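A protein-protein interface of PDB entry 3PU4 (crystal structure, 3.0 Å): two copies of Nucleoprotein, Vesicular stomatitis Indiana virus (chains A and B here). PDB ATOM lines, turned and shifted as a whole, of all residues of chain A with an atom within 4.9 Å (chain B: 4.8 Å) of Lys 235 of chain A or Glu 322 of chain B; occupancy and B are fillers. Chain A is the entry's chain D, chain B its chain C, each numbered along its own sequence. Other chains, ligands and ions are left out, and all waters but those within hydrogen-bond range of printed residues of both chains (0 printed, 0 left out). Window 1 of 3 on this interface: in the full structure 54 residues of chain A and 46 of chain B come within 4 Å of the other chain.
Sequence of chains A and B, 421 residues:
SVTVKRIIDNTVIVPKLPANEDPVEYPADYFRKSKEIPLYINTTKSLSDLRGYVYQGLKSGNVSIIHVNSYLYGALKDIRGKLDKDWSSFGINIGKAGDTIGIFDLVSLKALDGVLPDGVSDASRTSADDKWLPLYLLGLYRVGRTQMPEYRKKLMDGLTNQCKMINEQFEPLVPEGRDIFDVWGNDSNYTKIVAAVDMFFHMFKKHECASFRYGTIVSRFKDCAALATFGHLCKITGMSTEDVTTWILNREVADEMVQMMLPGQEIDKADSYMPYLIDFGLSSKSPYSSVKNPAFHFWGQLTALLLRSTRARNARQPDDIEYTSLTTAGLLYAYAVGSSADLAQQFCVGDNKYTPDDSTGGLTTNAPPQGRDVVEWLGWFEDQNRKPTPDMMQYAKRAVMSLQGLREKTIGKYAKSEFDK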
ATOM      1  N   GLY A 231      21.647  -9.212  20.404  1.00  0.00           N
ATOM      2  CA  GLY A 231      22.982  -8.929  20.882  1.00  0.00           C
ATOM      3  C   GLY A 231      23.970  -8.766  19.746  1.00  0.00           C
ATOM      4  O   GLY A 231      24.737  -7.819  19.743  1.00  0.00           O
ATOM      5  N   HIS A 232      23.965  -9.674  18.778  1.00  0.00           N
ATOM      6  CA  HIS A 232      24.905  -9.566  17.669  1.00  0.00           C
ATOM      7  C   HIS A 232      24.648  -8.320  16.848  1.00  0.00           C
ATOM      8  O   HIS A 232      25.582  -7.671  16.376  1.00  0.00           O
ATOM      9  CB  HIS A 232      24.843 -10.793  16.774  1.00  0.00           C
ATOM     10  CG  HIS A 232      25.341 -12.031  17.437  1.00  0.00           C
ATOM     11  ND1 HIS A 232      25.136 -13.291  16.919  1.00  0.00           N
ATOM     12  CD2 HIS A 232      26.027 -12.205  18.589  1.00  0.00           C
ATOM     13  CE1 HIS A 232      25.679 -14.187  17.721  1.00  0.00           C
ATOM     14  NE2 HIS A 232      26.221 -13.555  18.746  1.00  0.00           N
ATOM     15  N   LEU A 233      23.379  -7.987  16.687  1.00  0.00           N
ATOM     16  CA  LEU A 233      23.010  -6.831  15.903  1.00  0.00           C
ATOM     17  C   LEU A 233      23.644  -5.548  16.472  1.00  0.00           C
ATOM     18  O   LEU A 233      24.180  -4.697  15.744  1.00  0.00           O
ATOM     19  CB  LEU A 233      21.490  -6.716  15.842  1.00  0.00           C
ATOM     20  CG  LEU A 233      20.977  -5.807  14.737  1.00  0.00           C
ATOM     21  CD1 LEU A 233      21.784  -6.055  13.478  1.00  0.00           C
ATOM     22  CD2 LEU A 233      19.488  -6.027  14.524  1.00  0.00           C
ATOM     23  N   CYS A 234      23.597  -5.412  17.786  1.00  0.00           N
ATOM     24  CA  CYS A 234      24.187  -4.243  18.414  1.00  0.00           C
ATOM     25  C   CYS A 234      25.678  -4.259  18.207  1.00  0.00           C
ATOM     26  O   CYS A 234      26.248  -3.276  17.779  1.00  0.00           O
ATOM     27  CB  CYS A 234      23.893  -4.218  19.902  1.00  0.00           C
ATOM     28  SG  CYS A 234      22.148  -4.228  20.267  1.00  0.00           S
ATOM     29  N   LYS A 235      26.312  -5.377  18.520  1.00  0.00           N
ATOM     30  CA  LYS A 235      27.753  -5.469  18.420  1.00  0.00           C
ATOM     31  C   LYS A 235      28.199  -5.183  17.001  1.00  0.00           C
ATOM     32  O   LYS A 235      29.285  -4.665  16.773  1.00  0.00           O
ATOM     33  CB  LYS A 235      28.229  -6.855  18.848  1.00  0.00           C
ATOM     34  CG  LYS A 235      28.337  -7.026  20.343  1.00  0.00           C
ATOM     35  CD  LYS A 235      29.550  -6.294  20.856  1.00  0.00           C
ATOM     36  CE  LYS A 235      29.591  -6.219  22.385  1.00  0.00           C
ATOM     37  NZ  LYS A 235      30.043  -7.474  23.057  1.00  0.00           N
ATOM     38  N   ILE A 236      27.347  -5.505  16.041  1.00  0.00           N
ATOM     39  CA  ILE A 236      27.790  -5.548  14.657  1.00  0.00           C
ATOM     40  C   ILE A 236      27.532  -4.239  13.930  1.00  0.00           C
ATOM     41  O   ILE A 236      28.122  -3.991  12.878  1.00  0.00           O
ATOM     42  CB  ILE A 236      27.155  -6.731  13.915  1.00  0.00           C
ATOM     43  CG1 ILE A 236      28.032  -7.168  12.762  1.00  0.00           C
ATOM     44  CG2 ILE A 236      25.815  -6.351  13.397  1.00  0.00           C
ATOM     45  CD1 ILE A 236      27.698  -6.457  11.500  1.00  0.00           C
ATOM     46  N   THR A 237      26.660  -3.409  14.502  1.00  0.00           N
ATOM     47  CA  THR A 237      26.397  -2.076  13.964  1.00  0.00           C
ATOM     48  C   THR A 237      27.109  -1.005  14.776  1.00  0.00           C
ATOM     49  O   THR A 237      27.305   0.118  14.324  1.00  0.00           O
ATOM     50  CB  THR A 237      24.914  -1.702  14.025  1.00  0.00           C
ATOM     51  OG1 THR A 237      24.540  -1.535  15.399  1.00  0.00           O
ATOM     52  CG2 THR A 237      24.050  -2.747  13.351  1.00  0.00           C
ATOM     53  N   GLY A 238      27.465  -1.340  15.997  1.00  0.00           N
ATOM     54  CA  GLY A 238      28.106  -0.374  16.851  1.00  0.00           C
ATOM     55  C   GLY A 238      27.087   0.403  17.648  1.00  0.00           C
ATOM     56  O   GLY A 238      27.425   1.137  18.572  1.00  0.00           O
ATOM     57  N   ASP A 342      31.439   5.484  11.865  1.00  0.00           N
ATOM     58  CA  ASP A 342      31.516   6.226  13.130  1.00  0.00           C
ATOM     59  C   ASP A 342      32.572   7.285  12.936  1.00  0.00           C
ATOM     60  O   ASP A 342      32.316   8.468  13.089  1.00  0.00           O
ATOM     61  CB  ASP A 342      31.977   5.377  14.321  1.00  0.00           C
ATOM     62  CG  ASP A 342      31.331   4.008  14.373  1.00  0.00           C
ATOM     63  OD1 ASP A 342      32.103   3.004  14.360  1.00  0.00           O
ATOM     64  OD2 ASP A 342      30.075   3.931  14.458  1.00  0.00           O
ATOM     65  N   ARG A 372      23.351   8.380  11.630  1.00  0.00           N
ATOM     66  CA  ARG A 372      22.573   7.146  11.687  1.00  0.00           C
ATOM     67  C   ARG A 372      21.280   7.387  12.418  1.00  0.00           C
ATOM     68  O   ARG A 372      20.977   6.729  13.408  1.00  0.00           O
ATOM     69  CB  ARG A 372      23.346   6.048  12.412  1.00  0.00           C
ATOM     70  CG  ARG A 372      24.780   5.898  11.935  1.00  0.00           C
ATOM     71  CD  ARG A 372      25.558   4.906  12.787  1.00  0.00           C
ATOM     72  NE  ARG A 372      26.642   4.328  12.007  1.00  0.00           N
ATOM     73  CZ  ARG A 372      27.354   3.286  12.389  1.00  0.00           C
ATOM     74  NH1 ARG A 372      27.083   2.714  13.543  1.00  0.00           N
ATOM     75  NH2 ARG A 372      28.324   2.822  11.616  1.00  0.00           N
ATOM     76  N   GLU B 252      35.358   1.865  20.467  1.00  0.00           N
ATOM     77  CA  GLU B 252      35.717   0.578  21.057  1.00  0.00           C
ATOM     78  C   GLU B 252      37.139   0.136  20.764  1.00  0.00           C
ATOM     79  O   GLU B 252      37.664  -0.736  21.442  1.00  0.00           O
ATOM     80  CB  GLU B 252      34.713  -0.520  20.714  1.00  0.00           C
ATOM     81  CG  GLU B 252      34.204  -0.437  19.282  1.00  0.00           C
ATOM     82  CD  GLU B 252      33.190   0.691  19.059  1.00  0.00           C
ATOM     83  OE1 GLU B 252      31.988   0.483  19.362  1.00  0.00           O
ATOM     84  OE2 GLU B 252      33.598   1.777  18.575  1.00  0.00           O
ATOM     85  N   ASP B 320      31.528 -10.415  16.451  1.00  0.00           N
ATOM     86  CA  ASP B 320      30.870  -9.387  17.257  1.00  0.00           C
ATOM     87  C   ASP B 320      31.650  -8.077  17.392  1.00  0.00           C
ATOM     88  O   ASP B 320      31.713  -7.492  18.474  1.00  0.00           O
ATOM     89  CB  ASP B 320      30.541  -9.914  18.651  1.00  0.00           C
ATOM     90  CG  ASP B 320      29.339 -10.836  18.660  1.00  0.00           C
ATOM     91  OD1 ASP B 320      28.809 -11.134  17.559  1.00  0.00           O
ATOM     92  OD2 ASP B 320      28.935 -11.256  19.776  1.00  0.00           O
ATOM     93  N   ILE B 321      32.254  -7.635  16.298  1.00  0.00           N
ATOM     94  CA  ILE B 321      32.811  -6.302  16.237  1.00  0.00           C
ATOM     95  C   ILE B 321      32.166  -5.577  15.079  1.00  0.00           C
ATOM     96  O   ILE B 321      31.514  -6.176  14.231  1.00  0.00           O
ATOM     97  CB  ILE B 321      34.324  -6.297  16.023  1.00  0.00           C
ATOM     98  CG1 ILE B 321      34.685  -7.013  14.721  1.00  0.00           C
ATOM     99  CG2 ILE B 321      35.032  -6.895  17.219  1.00  0.00           C
ATOM    100  CD1 ILE B 321      36.153  -7.060  14.460  1.00  0.00           C
ATOM    101  N   GLU B 322      32.365  -4.274  15.040  1.00  0.00           N
ATOM    102  CA  GLU B 322      31.717  -3.442  14.054  1.00  0.00           C
ATOM    103  C   GLU B 322      32.526  -3.373  12.765  1.00  0.00           C
ATOM    104  O   GLU B 322      33.220  -2.384  12.520  1.00  0.00           O
ATOM    105  CB  GLU B 322      31.533  -2.051  14.628  1.00  0.00           C
ATOM    106  CG  GLU B 322      30.702  -1.166  13.740  1.00  0.00           C
ATOM    107  CD  GLU B 322      30.535   0.207  14.336  1.00  0.00           C
ATOM    108  OE1 GLU B 322      30.943   0.353  15.523  1.00  0.00           O
ATOM    109  OE2 GLU B 322      30.014   1.107  13.621  1.00  0.00           O
ATOM    110  N   TYR B 323      32.424  -4.422  11.945  1.00  0.00           N
ATOM    111  CA  TYR B 323      33.282  -4.569  10.775  1.00  0.00           C
ATOM    112  C   TYR B 323      33.322  -3.368   9.863  1.00  0.00           C
ATOM    113  O   TYR B 323      34.376  -2.778   9.683  1.00  0.00           O
ATOM    114  CB  TYR B 323      32.908  -5.784   9.967  1.00  0.00           C
ATOM    115  CG  TYR B 323      32.980  -7.072  10.721  1.00  0.00           C
ATOM    116  CD1 TYR B 323      31.834  -7.769  11.026  1.00  0.00           C
ATOM    117  CD2 TYR B 323      34.194  -7.598  11.112  1.00  0.00           C
ATOM    118  CE1 TYR B 323      31.880  -8.959  11.692  1.00  0.00           C
ATOM    119  CE2 TYR B 323      34.259  -8.792  11.799  1.00  0.00           C
ATOM    120  CZ  TYR B 323      33.095  -9.474  12.083  1.00  0.00           C
ATOM    121  OH  TYR B 323      33.142 -10.670  12.776  1.00  0.00           O
ATOM    122  N   THR B 324      32.183  -2.991   9.289  1.00  0.00           N
ATOM    123  CA  THR B 324      32.200  -1.955   8.230  1.00  0.00           C
ATOM    124  C   THR B 324      32.985  -0.723   8.624  1.00  0.00           C
ATOM    125  O   THR B 324      33.886  -0.283   7.901  1.00  0.00           O
ATOM    126  CB  THR B 324      30.817  -1.453   7.838  1.00  0.00           C
ATOM    127  OG1 THR B 324      30.273  -0.702   8.932  1.00  0.00           O
ATOM    128  CG2 THR B 324      29.914  -2.608   7.484  1.00  0.00           C
ATOM    129  N   SER B 325      32.626  -0.163   9.771  1.00  0.00           N
ATOM    130  CA  SER B 325      33.295   1.023  10.254  1.00  0.00           C
ATOM    131  C   SER B 325      34.763   0.747  10.582  1.00  0.00           C
ATOM    132  O   SER B 325      35.640   1.535  10.221  1.00  0.00           O
ATOM    133  CB  SER B 325      32.557   1.572  11.458  1.00  0.00           C
ATOM    134  OG  SER B 325      33.471   2.237  12.295  1.00  0.00           O
ATOM    135  N   LEU B 326      35.029  -0.378  11.243  1.00  0.00           N
ATOM    136  CA  LEU B 326      36.390  -0.728  11.611  1.00  0.00           C
ATOM    137  C   LEU B 326      37.265  -0.765  10.363  1.00  0.00           C
ATOM    138  O   LEU B 326      38.407  -0.321  10.371  1.00  0.00           O
ATOM    139  CB  LEU B 326      36.425  -2.062  12.350  1.00  0.00           C
ATOM    140  CG  LEU B 326      36.690  -2.004  13.860  1.00  0.00           C
ATOM    141  CD1 LEU B 326      37.038  -0.597  14.246  1.00  0.00           C
ATOM    142  CD2 LEU B 326      35.513  -2.503  14.693  1.00  0.00           C
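OG of Ser 325 of chain B sits at hydrogen-bond distance from OD1 of Asp 342 of chain A (2.6 Å). The side-chain carboxylate (OE2) of Glu 322 of chain B lies within salt-bridge range of the guanidinium group (NH2) of Arg 372 of chain A. OE2 of Glu 322 of chain B lies close to OD1 of Asp 342 of chain A (2.9 Å). The backbone carbonyl oxygen (O) of Thr 237 of chain A sits close to the side-chain carboxylate (OE2) of Glu 322 of chain B, at 3.0 Å.
The side-chain hydroxyl (OG1) of Thr 237 of chain A is in hydrogen-bond range of the backbone carbonyl oxygen (O) of Cys 234 of chain A, 3.4 Å away. O of Thr 237 of chain A lies within hydrogen-bond range of NH1 of Arg 372 of chain A, 2.7 Å away. O of Leu 233 of chain A sits close to OG1 of Thr 237 of chain A (3.2 Å). NH1 of Arg 372 of chain A is in salt-bridge range of OD2 of Asp 342 of chain A, at 3.4 Å.
Among the printed residues, pairs that only touch across the chains: His 232 of chain A with Asp 320 of chain B (3.2 Å), Gly 238 of chain A with Glu 322 of chain B (3.2 Å), Lys 235 of chain A with Asp 320 of chain B (3.4 Å), Lys 235 of chain A with Ile 321 of chain B (3.5 Å), Lys 235 of chain A with Glu 322 of chain B (3.6 Å), Ile 236 of chain A with Ile 321 of chain B (3.8 Å) and Ile 236 of chain A with Glu 322 of chain B (3.8 Å).
Printed residues of chain B within 4 Å of His 232 of chain A: Asp 320. Of chain B, only Asp 320, Ile 321 and Glu 322 come within 4 Å of Lys 235 of chain A. Of the printed residues of chain B, Ile 236 of chain A touches Ile 321 and Glu 322. Printed residues of chain B within 4 Å of Thr 237 of chain A: Glu 322. Of the printed residues of chain B, Arg 372 of chain A touches Glu 322. Of chain A, only Lys 235, Ile 236, Thr 237, Gly 238, Asp 342 and Arg 372 come within 4 Å of Glu 322 of chain B. Printed residues of chain A within 4 Å of Ser 325 of chain B: Asp 342.
Of the 8 printed residues of chain B, 4 touch a printed residue of chain A. Hydrophobic or aromatic side chains of chain A within 4 Å of the printed part of chain B: His 232 and Ile 236. Along chain A the printed residues that touch a printed residue of chain B span positions 232 to 372. Among the printed residues, Asp or Glu carboxylates within 4 Å of a Lys or Arg side-chain nitrogen of the other chain: Arg 372 of chain A with Glu 322 of chain B (3.1 Å).
No position is printed for both chains. Of the 11 pairs that touch across the chains among the printed residues, none has its exchanged pair printed and touching as well.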
